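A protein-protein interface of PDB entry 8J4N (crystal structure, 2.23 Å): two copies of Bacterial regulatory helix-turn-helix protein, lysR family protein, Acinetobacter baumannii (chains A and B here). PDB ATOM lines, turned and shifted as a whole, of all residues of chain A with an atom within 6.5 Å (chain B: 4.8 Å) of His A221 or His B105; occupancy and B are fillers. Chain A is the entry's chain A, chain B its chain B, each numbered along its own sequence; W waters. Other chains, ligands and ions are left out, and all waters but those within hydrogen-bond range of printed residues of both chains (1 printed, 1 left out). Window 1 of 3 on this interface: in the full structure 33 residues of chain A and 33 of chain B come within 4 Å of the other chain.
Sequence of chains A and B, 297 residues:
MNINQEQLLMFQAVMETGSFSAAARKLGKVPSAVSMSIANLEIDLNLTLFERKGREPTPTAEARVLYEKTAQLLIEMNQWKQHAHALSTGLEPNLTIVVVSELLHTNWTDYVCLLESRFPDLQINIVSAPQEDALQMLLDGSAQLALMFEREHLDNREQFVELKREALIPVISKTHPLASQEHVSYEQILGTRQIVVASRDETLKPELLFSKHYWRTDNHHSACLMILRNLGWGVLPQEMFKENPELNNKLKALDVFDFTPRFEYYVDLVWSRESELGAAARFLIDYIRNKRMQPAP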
ATOM      1  N   LEU A 104      22.761 -14.823  -0.676  1.00  0.00           N
ATOM      2  CA  LEU A 104      23.703 -15.581  -1.498  1.00  0.00           C
ATOM      3  C   LEU A 104      23.392 -15.447  -2.987  1.00  0.00           C
ATOM      4  O   LEU A 104      24.309 -15.335  -3.809  1.00  0.00           O
ATOM      5  CB  LEU A 104      23.697 -17.051  -1.073  1.00  0.00           C
ATOM      6  CG  LEU A 104      25.008 -17.823  -1.210  1.00  0.00           C
ATOM      7  CD1 LEU A 104      26.131 -17.123  -0.461  1.00  0.00           C
ATOM      8  CD2 LEU A 104      24.838 -19.247  -0.698  1.00  0.00           C
ATOM      9  N   HIS A 105      22.109 -15.458  -3.353  1.00  0.00           N
ATOM     10  CA  HIS A 105      21.690 -15.410  -4.749  1.00  0.00           C
ATOM     11  C   HIS A 105      21.250 -14.012  -5.172  1.00  0.00           C
ATOM     12  O   HIS A 105      20.343 -13.858  -5.999  1.00  0.00           O
ATOM     13  CB  HIS A 105      20.597 -16.447  -4.993  1.00  0.00           C
ATOM     14  CG  HIS A 105      21.066 -17.855  -4.785  1.00  0.00           C
ATOM     15  ND1 HIS A 105      21.489 -18.661  -5.820  1.00  0.00           N
ATOM     16  CD2 HIS A 105      21.217 -18.586  -3.654  1.00  0.00           C
ATOM     17  CE1 HIS A 105      21.859 -19.835  -5.340  1.00  0.00           C
ATOM     18  NE2 HIS A 105      21.705 -19.815  -4.028  1.00  0.00           N
ATOM     19  N   VAL A 197      12.223 -19.004   3.013  1.00  0.00           N
ATOM     20  CA  VAL A 197      13.674 -18.920   3.143  1.00  0.00           C
ATOM     21  C   VAL A 197      13.988 -18.077   4.371  1.00  0.00           C
ATOM     22  O   VAL A 197      13.639 -16.893   4.427  1.00  0.00           O
ATOM     23  CB  VAL A 197      14.322 -18.324   1.885  1.00  0.00           C
ATOM     24  CG1 VAL A 197      15.832 -18.233   2.064  1.00  0.00           C
ATOM     25  CG2 VAL A 197      13.984 -19.160   0.669  1.00  0.00           C
ATOM     26  N   THR A 217      13.530 -23.417   4.560  1.00  0.00           N
ATOM     27  CA  THR A 217      14.856 -23.687   4.032  1.00  0.00           C
ATOM     28  C   THR A 217      15.707 -22.448   4.261  1.00  0.00           C
ATOM     29  O   THR A 217      15.185 -21.358   4.501  1.00  0.00           O
ATOM     30  CB  THR A 217      14.825 -24.044   2.543  1.00  0.00           C
ATOM     31  OG1 THR A 217      16.116 -24.519   2.141  1.00  0.00           O
ATOM     32  CG2 THR A 217      14.464 -22.833   1.720  1.00  0.00           C
ATOM     33  N   ASN A 219      18.255 -21.212   2.131  1.00  0.00           N
ATOM     34  CA  ASN A 219      18.787 -20.496   0.980  1.00  0.00           C
ATOM     35  C   ASN A 219      17.862 -20.674  -0.217  1.00  0.00           C
ATOM     36  O   ASN A 219      17.048 -21.598  -0.273  1.00  0.00           O
ATOM     37  CB  ASN A 219      20.217 -20.936   0.640  1.00  0.00           C
ATOM     38  CG  ASN A 219      20.271 -22.238  -0.126  1.00  0.00           C
ATOM     39  OD1 ASN A 219      20.414 -22.239  -1.350  1.00  0.00           O
ATOM     40  ND2 ASN A 219      20.178 -23.353   0.586  1.00  0.00           N
ATOM     41  N   HIS A 220      18.005 -19.761  -1.182  1.00  0.00           N
ATOM     42  CA  HIS A 220      17.027 -19.639  -2.261  1.00  0.00           C
ATOM     43  C   HIS A 220      17.204 -20.714  -3.326  1.00  0.00           C
ATOM     44  O   HIS A 220      16.247 -21.038  -4.037  1.00  0.00           O
ATOM     45  CB  HIS A 220      17.118 -18.248  -2.888  1.00  0.00           C
ATOM     46  CG  HIS A 220      16.663 -17.149  -1.979  1.00  0.00           C
ATOM     47  ND1 HIS A 220      15.339 -16.945  -1.651  1.00  0.00           N
ATOM     48  CD2 HIS A 220      17.365 -16.210  -1.302  1.00  0.00           C
ATOM     49  CE1 HIS A 220      15.244 -15.916  -0.827  1.00  0.00           C
ATOM     50  NE2 HIS A 220      16.459 -15.454  -0.598  1.00  0.00           N
ATOM     51  N   HIS A 221      18.410 -21.267  -3.464  1.00  0.00           N
ATOM     52  CA  HIS A 221      18.604 -22.378  -4.392  1.00  0.00           C
ATOM     53  C   HIS A 221      17.797 -23.591  -3.951  1.00  0.00           C
ATOM     54  O   HIS A 221      17.092 -24.209  -4.755  1.00  0.00           O
ATOM     55  CB  HIS A 221      20.088 -22.730  -4.502  1.00  0.00           C
ATOM     56  CG  HIS A 221      20.346 -24.035  -5.195  1.00  0.00           C
ATOM     57  ND1 HIS A 221      20.172 -24.210  -6.552  1.00  0.00           N
ATOM     58  CD2 HIS A 221      20.753 -25.233  -4.712  1.00  0.00           C
ATOM     59  CE1 HIS A 221      20.466 -25.456  -6.875  1.00  0.00           C
ATOM     60  NE2 HIS A 221      20.821 -26.098  -5.778  1.00  0.00           N
ATOM     61  N   SER A 222      17.895 -23.945  -2.669  1.00  0.00           N
ATOM     62  CA  SER A 222      17.095 -25.043  -2.139  1.00  0.00           C
ATOM     63  C   SER A 222      15.606 -24.771  -2.310  1.00  0.00           C
ATOM     64  O   SER A 222      14.845 -25.665  -2.704  1.00  0.00           O
ATOM     65  CB  SER A 222      17.440 -25.269  -0.669  1.00  0.00           C
ATOM     66  OG  SER A 222      18.779 -25.703  -0.528  1.00  0.00           O
ATOM     67  N   ALA A 223      15.170 -23.540  -2.024  1.00  0.00           N
ATOM     68  CA  ALA A 223      13.763 -23.196  -2.203  1.00  0.00           C
ATOM     69  C   ALA A 223      13.355 -23.305  -3.666  1.00  0.00           C
ATOM     70  O   ALA A 223      12.287 -23.840  -3.987  1.00  0.00           O
ATOM     71  CB  ALA A 223      13.493 -21.788  -1.678  1.00  0.00           C
ATOM     72  N   CYS A 224      14.202 -22.801  -4.572  1.00  0.00           N
ATOM     73  CA  CYS A 224      13.880 -22.846  -5.996  1.00  0.00           C
ATOM     74  C   CYS A 224      13.748 -24.280  -6.494  1.00  0.00           C
ATOM     75  O   CYS A 224      12.838 -24.590  -7.273  1.00  0.00           O
ATOM     76  CB  CYS A 224      14.938 -22.092  -6.804  1.00  0.00           C
ATOM     77  SG  CYS A 224      14.571 -21.963  -8.575  1.00  0.00           S
ATOM     78  N   LEU A 225      14.640 -25.171  -6.049  1.00  0.00           N
ATOM     79  CA  LEU A 225      14.552 -26.575  -6.448  1.00  0.00           C
ATOM     80  C   LEU A 225      13.206 -27.184  -6.065  1.00  0.00           C
ATOM     81  O   LEU A 225      12.612 -27.938  -6.845  1.00  0.00           O
ATOM     82  CB  LEU A 225      15.689 -27.377  -5.816  1.00  0.00           C
ATOM     83  CG  LEU A 225      17.080 -27.266  -6.438  1.00  0.00           C
ATOM     84  CD1 LEU A 225      18.072 -28.095  -5.643  1.00  0.00           C
ATOM     85  CD2 LEU A 225      17.067 -27.716  -7.892  1.00  0.00           C
ATOM     86  N   MET A 226      12.708 -26.864  -4.869  1.00  0.00           N
ATOM     87  CA  MET A 226      11.459 -27.454  -4.398  1.00  0.00           C
ATOM     88  C   MET A 226      10.246 -26.790  -5.039  1.00  0.00           C
ATOM     89  O   MET A 226       9.225 -27.454  -5.256  1.00  0.00           O
ATOM     90  CB  MET A 226      11.398 -27.374  -2.873  1.00  0.00           C
ATOM     91  CG  MET A 226      12.302 -28.395  -2.196  1.00  0.00           C
ATOM     92  SD  MET A 226      12.177 -28.422  -0.399  1.00  0.00           S
ATOM     93  CE  MET A 226      12.708 -26.761   0.001  1.00  0.00           C
ATOM     94  N   LEU A 236      11.625 -15.497  -4.433  1.00  0.00           N
ATOM     95  CA  LEU A 236      12.979 -15.645  -4.950  1.00  0.00           C
ATOM     96  C   LEU A 236      13.505 -14.325  -5.422  1.00  0.00           C
ATOM     97  O   LEU A 236      12.746 -13.466  -5.911  1.00  0.00           O
ATOM     98  CB  LEU A 236      13.005 -16.656  -6.109  1.00  0.00           C
ATOM     99  CG  LEU A 236      12.551 -18.090  -5.832  1.00  0.00           C
ATOM    100  CD1 LEU A 236      12.768 -18.956  -7.063  1.00  0.00           C
ATOM    101  CD2 LEU A 236      13.275 -18.669  -4.630  1.00  0.00           C
ATOM    102  N   MET A 240      18.075 -14.251  -9.498  1.00  0.00           N
ATOM    103  CA  MET A 240      18.169 -15.648  -9.916  1.00  0.00           C
ATOM    104  C   MET A 240      17.721 -15.842 -11.357  1.00  0.00           C
ATOM    105  O   MET A 240      18.236 -16.724 -12.054  1.00  0.00           O
ATOM    106  CB  MET A 240      17.340 -16.541  -8.992  1.00  0.00           C
ATOM    107  CG  MET A 240      17.949 -16.750  -7.620  1.00  0.00           C
ATOM    108  SD  MET A 240      17.007 -17.930  -6.632  1.00  0.00           S
ATOM    109  CE  MET A 240      17.617 -19.483  -7.283  1.00  0.00           C
ATOM    110  N   LEU B 103      27.089 -30.374  -1.309  1.00  0.00           N
ATOM    111  CA  LEU B 103      26.093 -31.191  -1.991  1.00  0.00           C
ATOM    112  C   LEU B 103      24.831 -30.418  -2.350  1.00  0.00           C
ATOM    113  O   LEU B 103      23.869 -31.021  -2.835  1.00  0.00           O
ATOM    114  CB  LEU B 103      25.718 -32.397  -1.125  1.00  0.00           C
ATOM    115  CG  LEU B 103      26.877 -33.329  -0.747  1.00  0.00           C
ATOM    116  CD1 LEU B 103      26.372 -34.550   0.006  1.00  0.00           C
ATOM    117  CD2 LEU B 103      27.684 -33.748  -1.971  1.00  0.00           C
ATOM    118  N   LEU B 104      24.809 -29.104  -2.126  1.00  0.00           N
ATOM    119  CA  LEU B 104      23.595 -28.329  -2.364  1.00  0.00           C
ATOM    120  C   LEU B 104      23.218 -28.325  -3.839  1.00  0.00           C
ATOM    121  O   LEU B 104      22.040 -28.467  -4.185  1.00  0.00           O
ATOM    122  CB  LEU B 104      23.776 -26.897  -1.861  1.00  0.00           C
ATOM    123  CG  LEU B 104      23.691 -26.688  -0.354  1.00  0.00           C
ATOM    124  CD1 LEU B 104      24.429 -25.416   0.065  1.00  0.00           C
ATOM    125  CD2 LEU B 104      22.235 -26.657   0.093  1.00  0.00           C
ATOM    126  N   HIS B 105      24.201 -28.163  -4.721  1.00  0.00           N
ATOM    127  CA  HIS B 105      23.957 -28.084  -6.154  1.00  0.00           C
ATOM    128  C   HIS B 105      24.097 -29.444  -6.827  1.00  0.00           C
ATOM    129  O   HIS B 105      24.458 -29.531  -8.008  1.00  0.00           O
ATOM    130  CB  HIS B 105      24.890 -27.041  -6.760  1.00  0.00           C
ATOM    131  CG  HIS B 105      24.650 -25.666  -6.214  1.00  0.00           C
ATOM    132  ND1 HIS B 105      25.322 -25.177  -5.113  1.00  0.00           N
ATOM    133  CD2 HIS B 105      23.780 -24.697  -6.582  1.00  0.00           C
ATOM    134  CE1 HIS B 105      24.891 -23.959  -4.841  1.00  0.00           C
ATOM    135  NE2 HIS B 105      23.956 -23.643  -5.717  1.00  0.00           N
ATOM    136  N   THR B 106      23.822 -30.512  -6.078  1.00  0.00           N
ATOM    137  CA  THR B 106      23.585 -31.851  -6.591  1.00  0.00           C
ATOM    138  C   THR B 106      22.086 -32.149  -6.518  1.00  0.00           C
ATOM    139  O   THR B 106      21.268 -31.262  -6.257  1.00  0.00           O
ATOM    140  CB  THR B 106      24.421 -32.879  -5.821  1.00  0.00           C
ATOM    141  OG1 THR B 106      23.861 -33.081  -4.515  1.00  0.00           O
ATOM    142  CG2 THR B 106      25.866 -32.410  -5.700  1.00  0.00           C
ATOM    143  N   ASN B 107      21.728 -33.413  -6.723  1.00  0.00           N
ATOM    144  CA  ASN B 107      20.355 -33.823  -7.013  1.00  0.00           C
ATOM    145  C   ASN B 107      19.767 -34.548  -5.804  1.00  0.00           C
ATOM    146  O   ASN B 107      19.908 -35.763  -5.677  1.00  0.00           O
ATOM    147  CB  ASN B 107      20.358 -34.704  -8.262  1.00  0.00           C
ATOM    148  CG  ASN B 107      18.972 -35.138  -8.699  1.00  0.00           C
ATOM    149  OD1 ASN B 107      17.992 -35.050  -7.954  1.00  0.00           O
ATOM    150  ND2 ASN B 107      18.880 -35.577  -9.945  1.00  0.00           N
ATOM    151  N   ASN B 219      30.616 -22.842  -1.154  1.00  0.00           N
ATOM    152  CA  ASN B 219      29.591 -23.484  -1.964  1.00  0.00           C
ATOM    153  C   ASN B 219      29.846 -23.199  -3.438  1.00  0.00           C
ATOM    154  O   ASN B 219      30.576 -22.273  -3.799  1.00  0.00           O
ATOM    155  CB  ASN B 219      28.182 -23.041  -1.553  1.00  0.00           C
ATOM    156  CG  ASN B 219      27.818 -21.672  -2.076  1.00  0.00           C
ATOM    157  OD1 ASN B 219      27.121 -21.549  -3.083  1.00  0.00           O
ATOM    158  ND2 ASN B 219      28.274 -20.634  -1.389  1.00  0.00           N
ATOM    159  N   HIS B 220      29.224 -24.019  -4.285  1.00  0.00           N
ATOM    160  CA  HIS B 220      29.547 -24.036  -5.709  1.00  0.00           C
ATOM    161  C   HIS B 220      28.906 -22.885  -6.470  1.00  0.00           C
ATOM    162  O   HIS B 220      29.410 -22.497  -7.529  1.00  0.00           O
ATOM    163  CB  HIS B 220      29.122 -25.372  -6.321  1.00  0.00           C
ATOM    164  CG  HIS B 220      29.883 -26.546  -5.782  1.00  0.00           C
ATOM    165  ND1 HIS B 220      31.229 -26.739  -6.015  1.00  0.00           N
ATOM    166  CD2 HIS B 220      29.488 -27.576  -4.997  1.00  0.00           C
ATOM    167  CE1 HIS B 220      31.627 -27.843  -5.409  1.00  0.00           C
ATOM    168  NE2 HIS B 220      30.590 -28.370  -4.782  1.00  0.00           N
ATOM    169  N   HIS B 221      27.793 -22.344  -5.969  1.00  0.00           N
ATOM    170  CA  HIS B 221      27.202 -21.169  -6.599  1.00  0.00           C
ATOM    171  C   HIS B 221      28.153 -19.984  -6.520  1.00  0.00           C
ATOM    172  O   HIS B 221      28.397 -19.299  -7.518  1.00  0.00           O
ATOM    173  CB  HIS B 221      25.865 -20.826  -5.942  1.00  0.00           C
ATOM    174  CG  HIS B 221      25.362 -19.458  -6.289  1.00  0.00           C
ATOM    175  ND1 HIS B 221      25.381 -18.413  -5.391  1.00  0.00           N
ATOM    176  CD2 HIS B 221      24.828 -18.965  -7.431  1.00  0.00           C
ATOM    177  CE1 HIS B 221      24.883 -17.333  -5.966  1.00  0.00           C
ATOM    178  NE2 HIS B 221      24.539 -17.640  -7.204  1.00  0.00           N
ATOM    179  N   PRO B 237      29.844 -29.168  -9.910  1.00  0.00           N
ATOM    180  CA  PRO B 237      29.007 -30.344 -10.178  1.00  0.00           C
ATOM    181  C   PRO B 237      28.422 -30.310 -11.582  1.00  0.00           C
ATOM    182  O   PRO B 237      27.982 -29.269 -12.076  1.00  0.00           O
ATOM    183  CB  PRO B 237      27.910 -30.260  -9.110  1.00  0.00           C
ATOM    184  CG  PRO B 237      28.460 -29.359  -8.053  1.00  0.00           C
ATOM    185  CD  PRO B 237      29.364 -28.395  -8.755  1.00  0.00           C
ATOM    186  N   GLU B 239      25.681 -31.440 -12.324  1.00  0.00           N
ATOM    187  CA  GLU B 239      24.280 -31.073 -12.128  1.00  0.00           C
ATOM    188  C   GLU B 239      24.008 -29.602 -12.422  1.00  0.00           C
ATOM    189  O   GLU B 239      22.910 -29.256 -12.869  1.00  0.00           O
ATOM    190  CB  GLU B 239      23.882 -31.416 -10.689  1.00  0.00           C
ATOM    191  CG  GLU B 239      22.523 -30.916 -10.213  1.00  0.00           C
ATOM    192  CD  GLU B 239      21.358 -31.493 -10.990  1.00  0.00           C
ATOM    193  OE1 GLU B 239      21.376 -32.702 -11.291  1.00  0.00           O
ATOM    194  OE2 GLU B 239      20.395 -30.750 -11.262  1.00  0.00           O
ATOM    195  N   MET B 240      24.983 -28.719 -12.181  1.00  0.00           N
ATOM    196  CA  MET B 240      24.770 -27.295 -12.440  1.00  0.00           C
ATOM    197  C   MET B 240      24.543 -27.016 -13.919  1.00  0.00           C
ATOM    198  O   MET B 240      23.857 -26.050 -14.268  1.00  0.00           O
ATOM    199  CB  MET B 240      25.957 -26.473 -11.936  1.00  0.00           C
ATOM    200  CG  MET B 240      26.116 -26.477 -10.427  1.00  0.00           C
ATOM    201  SD  MET B 240      27.414 -25.353  -9.867  1.00  0.00           S
ATOM    202  CE  MET B 240      26.562 -23.782  -9.958  1.00  0.00           C
ATOM    203  N   GLU B 243      20.881 -27.937 -14.517  1.00  0.00           N
ATOM    204  CA  GLU B 243      19.978 -26.908 -14.009  1.00  0.00           C
ATOM    205  C   GLU B 243      20.058 -25.628 -14.825  1.00  0.00           C
ATOM    206  O   GLU B 243      19.047 -24.934 -14.982  1.00  0.00           O
ATOM    207  CB  GLU B 243      20.288 -26.607 -12.542  1.00  0.00           C
ATOM    208  CG  GLU B 243      19.969 -27.740 -11.597  1.00  0.00           C
ATOM    209  CD  GLU B 243      20.567 -27.538 -10.221  1.00  0.00           C
ATOM    210  OE1 GLU B 243      21.235 -26.504 -10.005  1.00  0.00           O
ATOM    211  OE2 GLU B 243      20.360 -28.408  -9.350  1.00  0.00           O
HETATM  212  O   HOH W   1      23.332 -21.931  -3.110  1.00  0.00           O
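Leu A104 touches Asn B219, and with the chains exchanged Asn A219 touches Leu B104. Leu A104 touches His B221, and with the chains exchanged His A221 touches Leu B104. His A105 touches His B221, and with the chains exchanged His A221 touches His B105. Positions printed for both chains: 104, 105, 219, 220, 221 and 240.
Hydrophobic or aromatic side chains of chain A within 4 Å of the printed part of chain B: Leu A104, His A105, His A221 and Leu A225. Hydrophobic or aromatic side chains of chain B within 4 Å of the printed part of chain A: Leu B104, His B105 and His B221. Along chain B the printed residues that touch a printed residue of chain A span positions 104 to 243. Among the printed residues, no Asp or Glu carboxylate lies within 4 Å of a Lys or Arg side-chain nitrogen of the other chain.
O of Leu B104 is in hydrogen-bond range of NE2 of His A221, 3.1 Å away.
His A221 touches three residues of chain B. Of the printed residues of chain A, His B105 touches His A221. Of the printed residues of chain A, His B221 touches Leu A104 (3.0 Å) and His A105 (3.5 Å). Of the printed residues of chain A, Asn B219 touches Leu A104 (3.8 Å). Printed residues of chain B within 4 Å of Leu A104: Asn B219 and His B221.
OG of Ser A222 is in hydrogen-bond range of ND2 of Asn A219 (3.0 Å). The side-chain amide oxygen (OD1) of Asn B219 sits at hydrogen-bond distance from the backbone NH (N) of His B221 (3.1 Å). The backbone NH (N) of His A221 sits at hydrogen-bond distance from the side-chain amide oxygen (OD1) of Asn A219 (3.1 Å).
Leu A104 touches Asn B219 (CD2 to ND2, 3.8 Å). Leu A104 touches His B221. ND1 of His A105 touches NE2 of His B221, at 3.5 Å. CD2 of Leu B104 touches ND2 of Asn A219 (3.9 Å). His B105 touches His A221. OE1 of Glu B243 touches CE1 of His A221, at 3.4 Å. Ser A222 touches Leu B104. Leu A225 touches Glu B243.
Water W1 lies within hydrogen-bond range of NE2 of His A105 (2.8 Å), NE2 of His B105 (3.2 Å) and OD1 of Asn A219 (3.4 Å).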
